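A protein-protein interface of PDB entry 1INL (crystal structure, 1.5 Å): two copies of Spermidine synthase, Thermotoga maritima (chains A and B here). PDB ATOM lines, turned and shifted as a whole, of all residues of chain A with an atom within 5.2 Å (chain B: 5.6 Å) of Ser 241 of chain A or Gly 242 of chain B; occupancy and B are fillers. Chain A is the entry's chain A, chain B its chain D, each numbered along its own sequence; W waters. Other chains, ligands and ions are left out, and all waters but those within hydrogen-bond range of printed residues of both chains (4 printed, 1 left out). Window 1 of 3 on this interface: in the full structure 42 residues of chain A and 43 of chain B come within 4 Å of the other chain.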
ATOM      1  N   TYR A  23     -29.894 -16.439  -6.491  1.00  0.00           N
ATOM      2  CA  TYR A  23     -28.482 -16.240  -6.781  1.00  0.00           C
ATOM      3  C   TYR A  23     -27.792 -17.594  -6.667  1.00  0.00           C
ATOM      4  O   TYR A  23     -28.368 -18.545  -6.132  1.00  0.00           O
ATOM      5  CB  TYR A  23     -27.856 -15.266  -5.780  1.00  0.00           C
ATOM      6  CG  TYR A  23     -28.441 -13.873  -5.807  1.00  0.00           C
ATOM      7  CD1 TYR A  23     -29.120 -13.397  -6.926  1.00  0.00           C
ATOM      8  CD2 TYR A  23     -28.287 -13.023  -4.718  1.00  0.00           C
ATOM      9  CE1 TYR A  23     -29.630 -12.103  -6.959  1.00  0.00           C
ATOM     10  CE2 TYR A  23     -28.788 -11.731  -4.739  1.00  0.00           C
ATOM     11  CZ  TYR A  23     -29.455 -11.277  -5.861  1.00  0.00           C
ATOM     12  OH  TYR A  23     -29.930  -9.987  -5.881  1.00  0.00           O
ATOM     13  N   ASP A 207     -19.958 -11.294 -10.646  1.00  0.00           N
ATOM     14  CA  ASP A 207     -19.697 -10.731  -9.328  1.00  0.00           C
ATOM     15  C   ASP A 207     -18.728 -11.576  -8.513  1.00  0.00           C
ATOM     16  O   ASP A 207     -18.890 -12.791  -8.417  1.00  0.00           O
ATOM     17  CB  ASP A 207     -21.011 -10.589  -8.553  1.00  0.00           C
ATOM     18  CG  ASP A 207     -21.717 -11.917  -8.356  1.00  0.00           C
ATOM     19  OD1 ASP A 207     -22.213 -12.479  -9.354  1.00  0.00           O
ATOM     20  OD2 ASP A 207     -21.769 -12.400  -7.208  1.00  0.00           O
ATOM     21  N   PHE A 209     -18.492 -12.358  -5.646  1.00  0.00           N
ATOM     22  CA  PHE A 209     -19.173 -12.607  -4.381  1.00  0.00           C
ATOM     23  C   PHE A 209     -19.884 -13.960  -4.472  1.00  0.00           C
ATOM     24  O   PHE A 209     -19.323 -14.976  -4.063  1.00  0.00           O
ATOM     25  CB  PHE A 209     -20.164 -11.465  -4.098  1.00  0.00           C
ATOM     26  CG  PHE A 209     -20.627 -11.390  -2.666  1.00  0.00           C
ATOM     27  CD1 PHE A 209     -21.971 -11.557  -2.348  1.00  0.00           C
ATOM     28  CD2 PHE A 209     -19.723 -11.137  -1.638  1.00  0.00           C
ATOM     29  CE1 PHE A 209     -22.416 -11.473  -1.026  1.00  0.00           C
ATOM     30  CE2 PHE A 209     -20.155 -11.050  -0.312  1.00  0.00           C
ATOM     31  CZ  PHE A 209     -21.507 -11.219  -0.006  1.00  0.00           C
ATOM     32  N   TYR A 210     -21.088 -13.993  -5.045  1.00  0.00           N
ATOM     33  CA  TYR A 210     -21.823 -15.254  -5.182  1.00  0.00           C
ATOM     34  C   TYR A 210     -21.201 -16.124  -6.265  1.00  0.00           C
ATOM     35  O   TYR A 210     -21.271 -17.353  -6.207  1.00  0.00           O
ATOM     36  CB  TYR A 210     -23.291 -15.001  -5.549  1.00  0.00           C
ATOM     37  CG  TYR A 210     -24.057 -14.235  -4.505  1.00  0.00           C
ATOM     38  CD1 TYR A 210     -24.356 -14.813  -3.271  1.00  0.00           C
ATOM     39  CD2 TYR A 210     -24.465 -12.923  -4.738  1.00  0.00           C
ATOM     40  CE1 TYR A 210     -25.038 -14.100  -2.292  1.00  0.00           C
ATOM     41  CE2 TYR A 210     -25.148 -12.200  -3.767  1.00  0.00           C
ATOM     42  CZ  TYR A 210     -25.428 -12.796  -2.547  1.00  0.00           C
ATOM     43  OH  TYR A 210     -26.077 -12.081  -1.573  1.00  0.00           O
ATOM     44  N   PHE A 235     -20.720  -0.664 -10.920  1.00  0.00           N
ATOM     45  CA  PHE A 235     -21.963  -0.862 -10.194  1.00  0.00           C
ATOM     46  C   PHE A 235     -23.007  -1.384 -11.179  1.00  0.00           C
ATOM     47  O   PHE A 235     -23.006  -1.022 -12.354  1.00  0.00           O
ATOM     48  CB  PHE A 235     -22.429   0.451  -9.558  1.00  0.00           C
ATOM     49  CG  PHE A 235     -21.519   0.950  -8.468  1.00  0.00           C
ATOM     50  CD1 PHE A 235     -21.521   0.342  -7.218  1.00  0.00           C
ATOM     51  CD2 PHE A 235     -20.647   2.012  -8.695  1.00  0.00           C
ATOM     52  CE1 PHE A 235     -20.665   0.781  -6.206  1.00  0.00           C
ATOM     53  CE2 PHE A 235     -19.789   2.457  -7.695  1.00  0.00           C
ATOM     54  CZ  PHE A 235     -19.798   1.840  -6.447  1.00  0.00           C
ATOM     55  N   TYR A 239     -28.033  -6.590 -10.620  1.00  0.00           N
ATOM     56  CA  TYR A 239     -27.348  -7.867 -10.834  1.00  0.00           C
ATOM     57  C   TYR A 239     -26.933  -8.370  -9.452  1.00  0.00           C
ATOM     58  O   TYR A 239     -26.764  -7.573  -8.526  1.00  0.00           O
ATOM     59  CB  TYR A 239     -26.112  -7.704 -11.730  1.00  0.00           C
ATOM     60  CG  TYR A 239     -26.372  -7.814 -13.223  1.00  0.00           C
ATOM     61  CD1 TYR A 239     -27.654  -8.044 -13.730  1.00  0.00           C
ATOM     62  CD2 TYR A 239     -25.327  -7.666 -14.131  1.00  0.00           C
ATOM     63  CE1 TYR A 239     -27.879  -8.116 -15.106  1.00  0.00           C
ATOM     64  CE2 TYR A 239     -25.541  -7.735 -15.500  1.00  0.00           C
ATOM     65  CZ  TYR A 239     -26.816  -7.958 -15.983  1.00  0.00           C
ATOM     66  OH  TYR A 239     -27.021  -8.008 -17.343  1.00  0.00           O
ATOM     67  N   PRO A 240     -26.743  -9.691  -9.297  1.00  0.00           N
ATOM     68  CA  PRO A 240     -26.355 -10.290  -8.013  1.00  0.00           C
ATOM     69  C   PRO A 240     -25.184  -9.598  -7.318  1.00  0.00           C
ATOM     70  O   PRO A 240     -24.085  -9.525  -7.869  1.00  0.00           O
ATOM     71  CB  PRO A 240     -26.008 -11.729  -8.400  1.00  0.00           C
ATOM     72  CG  PRO A 240     -26.939 -11.991  -9.550  1.00  0.00           C
ATOM     73  CD  PRO A 240     -26.814 -10.720 -10.351  1.00  0.00           C
ATOM     74  N   SER A 241     -25.458  -9.085  -6.114  1.00  0.00           N
ATOM     75  CA  SER A 241     -24.503  -8.380  -5.247  1.00  0.00           C
ATOM     76  C   SER A 241     -24.287  -6.902  -5.572  1.00  0.00           C
ATOM     77  O   SER A 241     -23.835  -6.143  -4.717  1.00  0.00           O
ATOM     78  CB  SER A 241     -23.144  -9.099  -5.185  1.00  0.00           C
ATOM     79  OG  SER A 241     -22.261  -8.651  -6.203  1.00  0.00           O
ATOM     80  N   GLY A 242     -24.599  -6.503  -6.803  1.00  0.00           N
ATOM     81  CA  GLY A 242     -24.418  -5.117  -7.204  1.00  0.00           C
ATOM     82  C   GLY A 242     -22.987  -4.751  -7.563  1.00  0.00           C
ATOM     83  O   GLY A 242     -22.712  -3.622  -7.969  1.00  0.00           O
ATOM     84  N   MET A 243     -22.073  -5.700  -7.393  1.00  0.00           N
ATOM     85  CA  MET A 243     -20.663  -5.497  -7.702  1.00  0.00           C
ATOM     86  C   MET A 243     -20.336  -6.365  -8.908  1.00  0.00           C
ATOM     87  O   MET A 243     -20.165  -7.580  -8.781  1.00  0.00           O
ATOM     88  CB  MET A 243     -19.805  -5.907  -6.503  1.00  0.00           C
ATOM     89  CG  MET A 243     -18.312  -5.775  -6.729  1.00  0.00           C
ATOM     90  SD  MET A 243     -17.391  -6.152  -5.228  1.00  0.00           S
ATOM     91  CE  MET A 243     -15.867  -5.337  -5.566  1.00  0.00           C
ATOM     92  N   GLY B 234     -18.965   3.152  -2.750  1.00  0.00           N
ATOM     93  CA  GLY B 234     -18.366   1.880  -2.417  1.00  0.00           C
ATOM     94  C   GLY B 234     -19.346   0.752  -2.640  1.00  0.00           C
ATOM     95  O   GLY B 234     -20.563   0.959  -2.623  1.00  0.00           O
ATOM     96  N   PHE B 235     -18.811  -0.429  -2.916  1.00  0.00           N
ATOM     97  CA  PHE B 235     -19.643  -1.605  -3.108  1.00  0.00           C
ATOM     98  C   PHE B 235     -20.088  -2.084  -1.736  1.00  0.00           C
ATOM     99  O   PHE B 235     -19.354  -1.957  -0.755  1.00  0.00           O
ATOM    100  CB  PHE B 235     -18.857  -2.703  -3.828  1.00  0.00           C
ATOM    101  CG  PHE B 235     -18.506  -2.360  -5.243  1.00  0.00           C
ATOM    102  CD1 PHE B 235     -19.473  -2.410  -6.241  1.00  0.00           C
ATOM    103  CD2 PHE B 235     -17.215  -1.972  -5.579  1.00  0.00           C
ATOM    104  CE1 PHE B 235     -19.157  -2.077  -7.559  1.00  0.00           C
ATOM    105  CE2 PHE B 235     -16.884  -1.637  -6.891  1.00  0.00           C
ATOM    106  CZ  PHE B 235     -17.859  -1.689  -7.885  1.00  0.00           C
ATOM    107  N   MET B 236     -21.329  -2.546  -1.660  1.00  0.00           N
ATOM    108  CA  MET B 236     -21.899  -3.056  -0.420  1.00  0.00           C
ATOM    109  C   MET B 236     -22.819  -4.161  -0.912  1.00  0.00           C
ATOM    110  O   MET B 236     -23.994  -3.939  -1.200  1.00  0.00           O
ATOM    111  CB  MET B 236     -22.687  -1.963   0.303  1.00  0.00           C
ATOM    112  CG  MET B 236     -22.651  -2.068   1.816  1.00  0.00           C
ATOM    113  SD  MET B 236     -23.145  -3.691   2.425  1.00  0.00           S
ATOM    114  CE  MET B 236     -21.549  -4.314   2.841  1.00  0.00           C
ATOM    115  N   THR B 237     -22.250  -5.359  -1.004  1.00  0.00           N
ATOM    116  CA  THR B 237     -22.930  -6.535  -1.536  1.00  0.00           C
ATOM    117  C   THR B 237     -24.281  -6.993  -0.989  1.00  0.00           C
ATOM    118  O   THR B 237     -24.947  -7.805  -1.633  1.00  0.00           O
ATOM    119  CB  THR B 237     -21.948  -7.712  -1.649  1.00  0.00           C
ATOM    120  OG1 THR B 237     -21.270  -7.895  -0.401  1.00  0.00           O
ATOM    121  CG2 THR B 237     -20.911  -7.422  -2.728  1.00  0.00           C
ATOM    122  N   THR B 238     -24.695  -6.498   0.177  1.00  0.00           N
ATOM    123  CA  THR B 238     -26.002  -6.875   0.723  1.00  0.00           C
ATOM    124  C   THR B 238     -26.916  -5.695   1.062  1.00  0.00           C
ATOM    125  O   THR B 238     -27.949  -5.873   1.708  1.00  0.00           O
ATOM    126  CB  THR B 238     -25.906  -7.828   1.942  1.00  0.00           C
ATOM    127  OG1 THR B 238     -24.959  -7.317   2.885  1.00  0.00           O
ATOM    128  CG2 THR B 238     -25.507  -9.229   1.502  1.00  0.00           C
ATOM    129  N   TYR B 239     -26.519  -4.488   0.668  1.00  0.00           N
ATOM    130  CA  TYR B 239     -27.356  -3.313   0.897  1.00  0.00           C
ATOM    131  C   TYR B 239     -28.139  -3.064  -0.393  1.00  0.00           C
ATOM    132  O   TYR B 239     -27.698  -3.458  -1.477  1.00  0.00           O
ATOM    133  CB  TYR B 239     -26.514  -2.083   1.255  1.00  0.00           C
ATOM    134  CG  TYR B 239     -26.196  -1.930   2.729  1.00  0.00           C
ATOM    135  CD1 TYR B 239     -26.656  -2.851   3.674  1.00  0.00           C
ATOM    136  CD2 TYR B 239     -25.413  -0.871   3.177  1.00  0.00           C
ATOM    137  CE1 TYR B 239     -26.336  -2.712   5.028  1.00  0.00           C
ATOM    138  CE2 TYR B 239     -25.087  -0.727   4.519  1.00  0.00           C
ATOM    139  CZ  TYR B 239     -25.547  -1.646   5.439  1.00  0.00           C
ATOM    140  OH  TYR B 239     -25.201  -1.493   6.762  1.00  0.00           O
ATOM    141  N   PRO B 240     -29.292  -2.381  -0.301  1.00  0.00           N
ATOM    142  CA  PRO B 240     -30.140  -2.085  -1.461  1.00  0.00           C
ATOM    143  C   PRO B 240     -29.389  -1.485  -2.648  1.00  0.00           C
ATOM    144  O   PRO B 240     -28.766  -0.431  -2.523  1.00  0.00           O
ATOM    145  CB  PRO B 240     -31.171  -1.115  -0.888  1.00  0.00           C
ATOM    146  CG  PRO B 240     -31.310  -1.592   0.531  1.00  0.00           C
ATOM    147  CD  PRO B 240     -29.870  -1.800   0.925  1.00  0.00           C
ATOM    148  N   SER B 241     -29.442  -2.200  -3.775  1.00  0.00           N
ATOM    149  CA  SER B 241     -28.800  -1.829  -5.048  1.00  0.00           C
ATOM    150  C   SER B 241     -27.318  -2.177  -5.143  1.00  0.00           C
ATOM    151  O   SER B 241     -26.769  -2.270  -6.244  1.00  0.00           O
ATOM    152  CB  SER B 241     -28.997  -0.342  -5.382  1.00  0.00           C
ATOM    153  OG  SER B 241     -27.962   0.460  -4.835  1.00  0.00           O
ATOM    154  N   GLY B 242     -26.669  -2.362  -3.996  1.00  0.00           N
ATOM    155  CA  GLY B 242     -25.252  -2.684  -3.993  1.00  0.00           C
ATOM    156  C   GLY B 242     -24.342  -1.488  -4.230  1.00  0.00           C
ATOM    157  O   GLY B 242     -23.117  -1.616  -4.172  1.00  0.00           O
ATOM    158  N   MET B 243     -24.935  -0.333  -4.518  1.00  0.00           N
ATOM    159  CA  MET B 243     -24.176   0.891  -4.760  1.00  0.00           C
ATOM    160  C   MET B 243     -24.408   1.814  -3.572  1.00  0.00           C
ATOM    161  O   MET B 243     -25.461   2.439  -3.464  1.00  0.00           O
ATOM    162  CB  MET B 243     -24.654   1.554  -6.054  1.00  0.00           C
ATOM    163  CG  MET B 243     -23.949   2.852  -6.399  1.00  0.00           C
ATOM    164  SD  MET B 243     -24.522   3.455  -7.983  1.00  0.00           S
ATOM    165  CE  MET B 243     -23.282   4.644  -8.362  1.00  0.00           C
ATOM    166  N   TRP B 244     -23.427   1.896  -2.680  1.00  0.00           N
ATOM    167  CA  TRP B 244     -23.582   2.735  -1.502  1.00  0.00           C
ATOM    168  C   TRP B 244     -22.781   4.018  -1.586  1.00  0.00           C
ATOM    169  O   TRP B 244     -21.680   4.043  -2.137  1.00  0.00           O
ATOM    170  CB  TRP B 244     -23.201   1.968  -0.233  1.00  0.00           C
ATOM    171  CG  TRP B 244     -24.092   2.301   0.922  1.00  0.00           C
ATOM    172  CD1 TRP B 244     -23.736   2.914   2.089  1.00  0.00           C
ATOM    173  CD2 TRP B 244     -25.495   2.047   1.013  1.00  0.00           C
ATOM    174  NE1 TRP B 244     -24.836   3.057   2.903  1.00  0.00           N
ATOM    175  CE2 TRP B 244     -25.929   2.533   2.265  1.00  0.00           C
ATOM    176  CE3 TRP B 244     -26.431   1.452   0.155  1.00  0.00           C
ATOM    177  CZ2 TRP B 244     -27.262   2.443   2.682  1.00  0.00           C
ATOM    178  CZ3 TRP B 244     -27.756   1.363   0.570  1.00  0.00           C
ATOM    179  CH2 TRP B 244     -28.157   1.858   1.824  1.00  0.00           C
HETATM  180  O   HOH W   1     -26.822  -9.554  -2.160  1.00  0.00           O
HETATM  181  O   HOH W   2     -24.489  -1.639  -7.721  1.00  0.00           O
HETATM  182  O   HOH W   3     -22.004  -4.122  -4.350  1.00  0.00           O
HETATM  183  O   HOH W   4     -27.758  -5.249  -7.266  1.00  0.00           O
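Thr 237 of chain B touches Phe 209 of chain A. Phe 235 of chain A touches Gly 234 of chain B. Phe 235 of chain A touches Phe 235 of chain B (CD1 to CE1, 3.4 Å). CD1 of Phe 235 of chain A touches O of Gly 242 of chain B (3.96 Å). Met 243 of chain B touches Phe 235 of chain A (CB to CD1, 3.6 Å). Ser 241 of chain A touches Thr 237 of chain B. Ser 241 of chain A touches Gly 242 of chain B. Gly 242 of chain A touches Phe 235 of chain B. Ser 241 of chain B touches Gly 242 of chain A. CB of Met 243 of chain A touches CD1 of Phe 235 of chain B (3.5 Å).
N of Met 243 of chain A sits close to OG of Ser 241 of chain A. N of Gly 234 of chain B lies within hydrogen-bond range of O of Trp 244 of chain B, 2.9 Å away. The backbone NH of Met 236 of chain B is in hydrogen-bond range of the backbone carbonyl oxygen of Gly 242 of chain B (3.2 Å). The side-chain hydroxyl (OG) of Ser 241 of chain B lies close to the backbone NH (N) of Met 243 of chain B, 3.1 Å away.
Water W1 bridges O of Thr 237 of chain B (2.6 Å) and OH of Tyr 210 of chain A (2.7 Å). Water W2 lies within hydrogen-bond range of the backbone carbonyl oxygen (O) of Gly 242 of chain A (2.7 Å), the backbone carbonyl oxygen (O) of Ser 241 of chain B (2.8 Å) and the backbone NH (N) of Met 243 of chain B (3.5 Å). Water W3 lies within hydrogen-bond range of O of Gly 242 of chain B (2.7 Å), O of Ser 241 of chain A (2.8 Å), N of Met 236 of chain B (3.2 Å) and N of Met 243 of chain A (3.4 Å). Water W4 lies within hydrogen-bond range of O of Tyr 239 of chain A (2.8 Å), O of Ser 241 of chain B (3.3 Å) and N of Gly 242 of chain A (3.4 Å).
Of chain B, only Thr 237 and Gly 242 come within 4 Å of Ser 241 of chain A. Printed residues of chain A within 4 Å of Gly 242 of chain B: Phe 235 and Ser 241. Of the printed residues of chain B, Phe 209 of chain A touches Thr 237. Printed residues of chain A within 4 Å of Met 243 of chain B: Phe 235 (3.6 Å). Printed residues of chain B within 4 Å of Gly 242 of chain A: Phe 235 and Ser 241. Of the printed residues of chain A, Gly 234 of chain B touches Phe 235. Tyr 210 of chain A touches none of the printed residues of chain B. Met 236 of chain B touches none of the printed residues of chain A. The nearest residue of chain A that does not touch Gly 242 of chain B is Gly 242 of chain A (4.1 Å). The nearest printed residue of chain A that does not touch Ser 241 of chain B is Ser 241 of chain A (5.1 Å).
Phe 235 of chain A touches its own counterpart, Phe 235 of chain B. Phe 235 of chain A touches Gly 242 of chain B, and with the chains exchanged Gly 242 of chain A touches Phe 235 of chain B. Phe 235 of chain A touches Met 243 of chain B, and with the chains exchanged Met 243 of chain A touches Phe 235 of chain B. Ser 241 of chain A touches Gly 242 of chain B, and with the chains exchanged Gly 242 of chain A touches Ser 241 of chain B. 6 positions are printed for both chains.
Of the 11 printed residues of chain B, 6 touch a printed residue of chain A. Printed residues of chain B that touch a printed residue of chain A: Gly 234, Phe 235, Thr 237, Ser 241, Gly 242 and Met 243. Hydrophobic or aromatic side chains of chain B within 4 Å of the printed part of chain A: Phe 235 and Met 243. Hydrophobic or aromatic side chains of chain A that line the printed part of chain B: Phe 209, Phe 235 and Met 243. Along chain A the printed residues that touch a printed residue of chain B span positions 209 to 243. Among the printed residues, 10 pairs touch across the chains.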
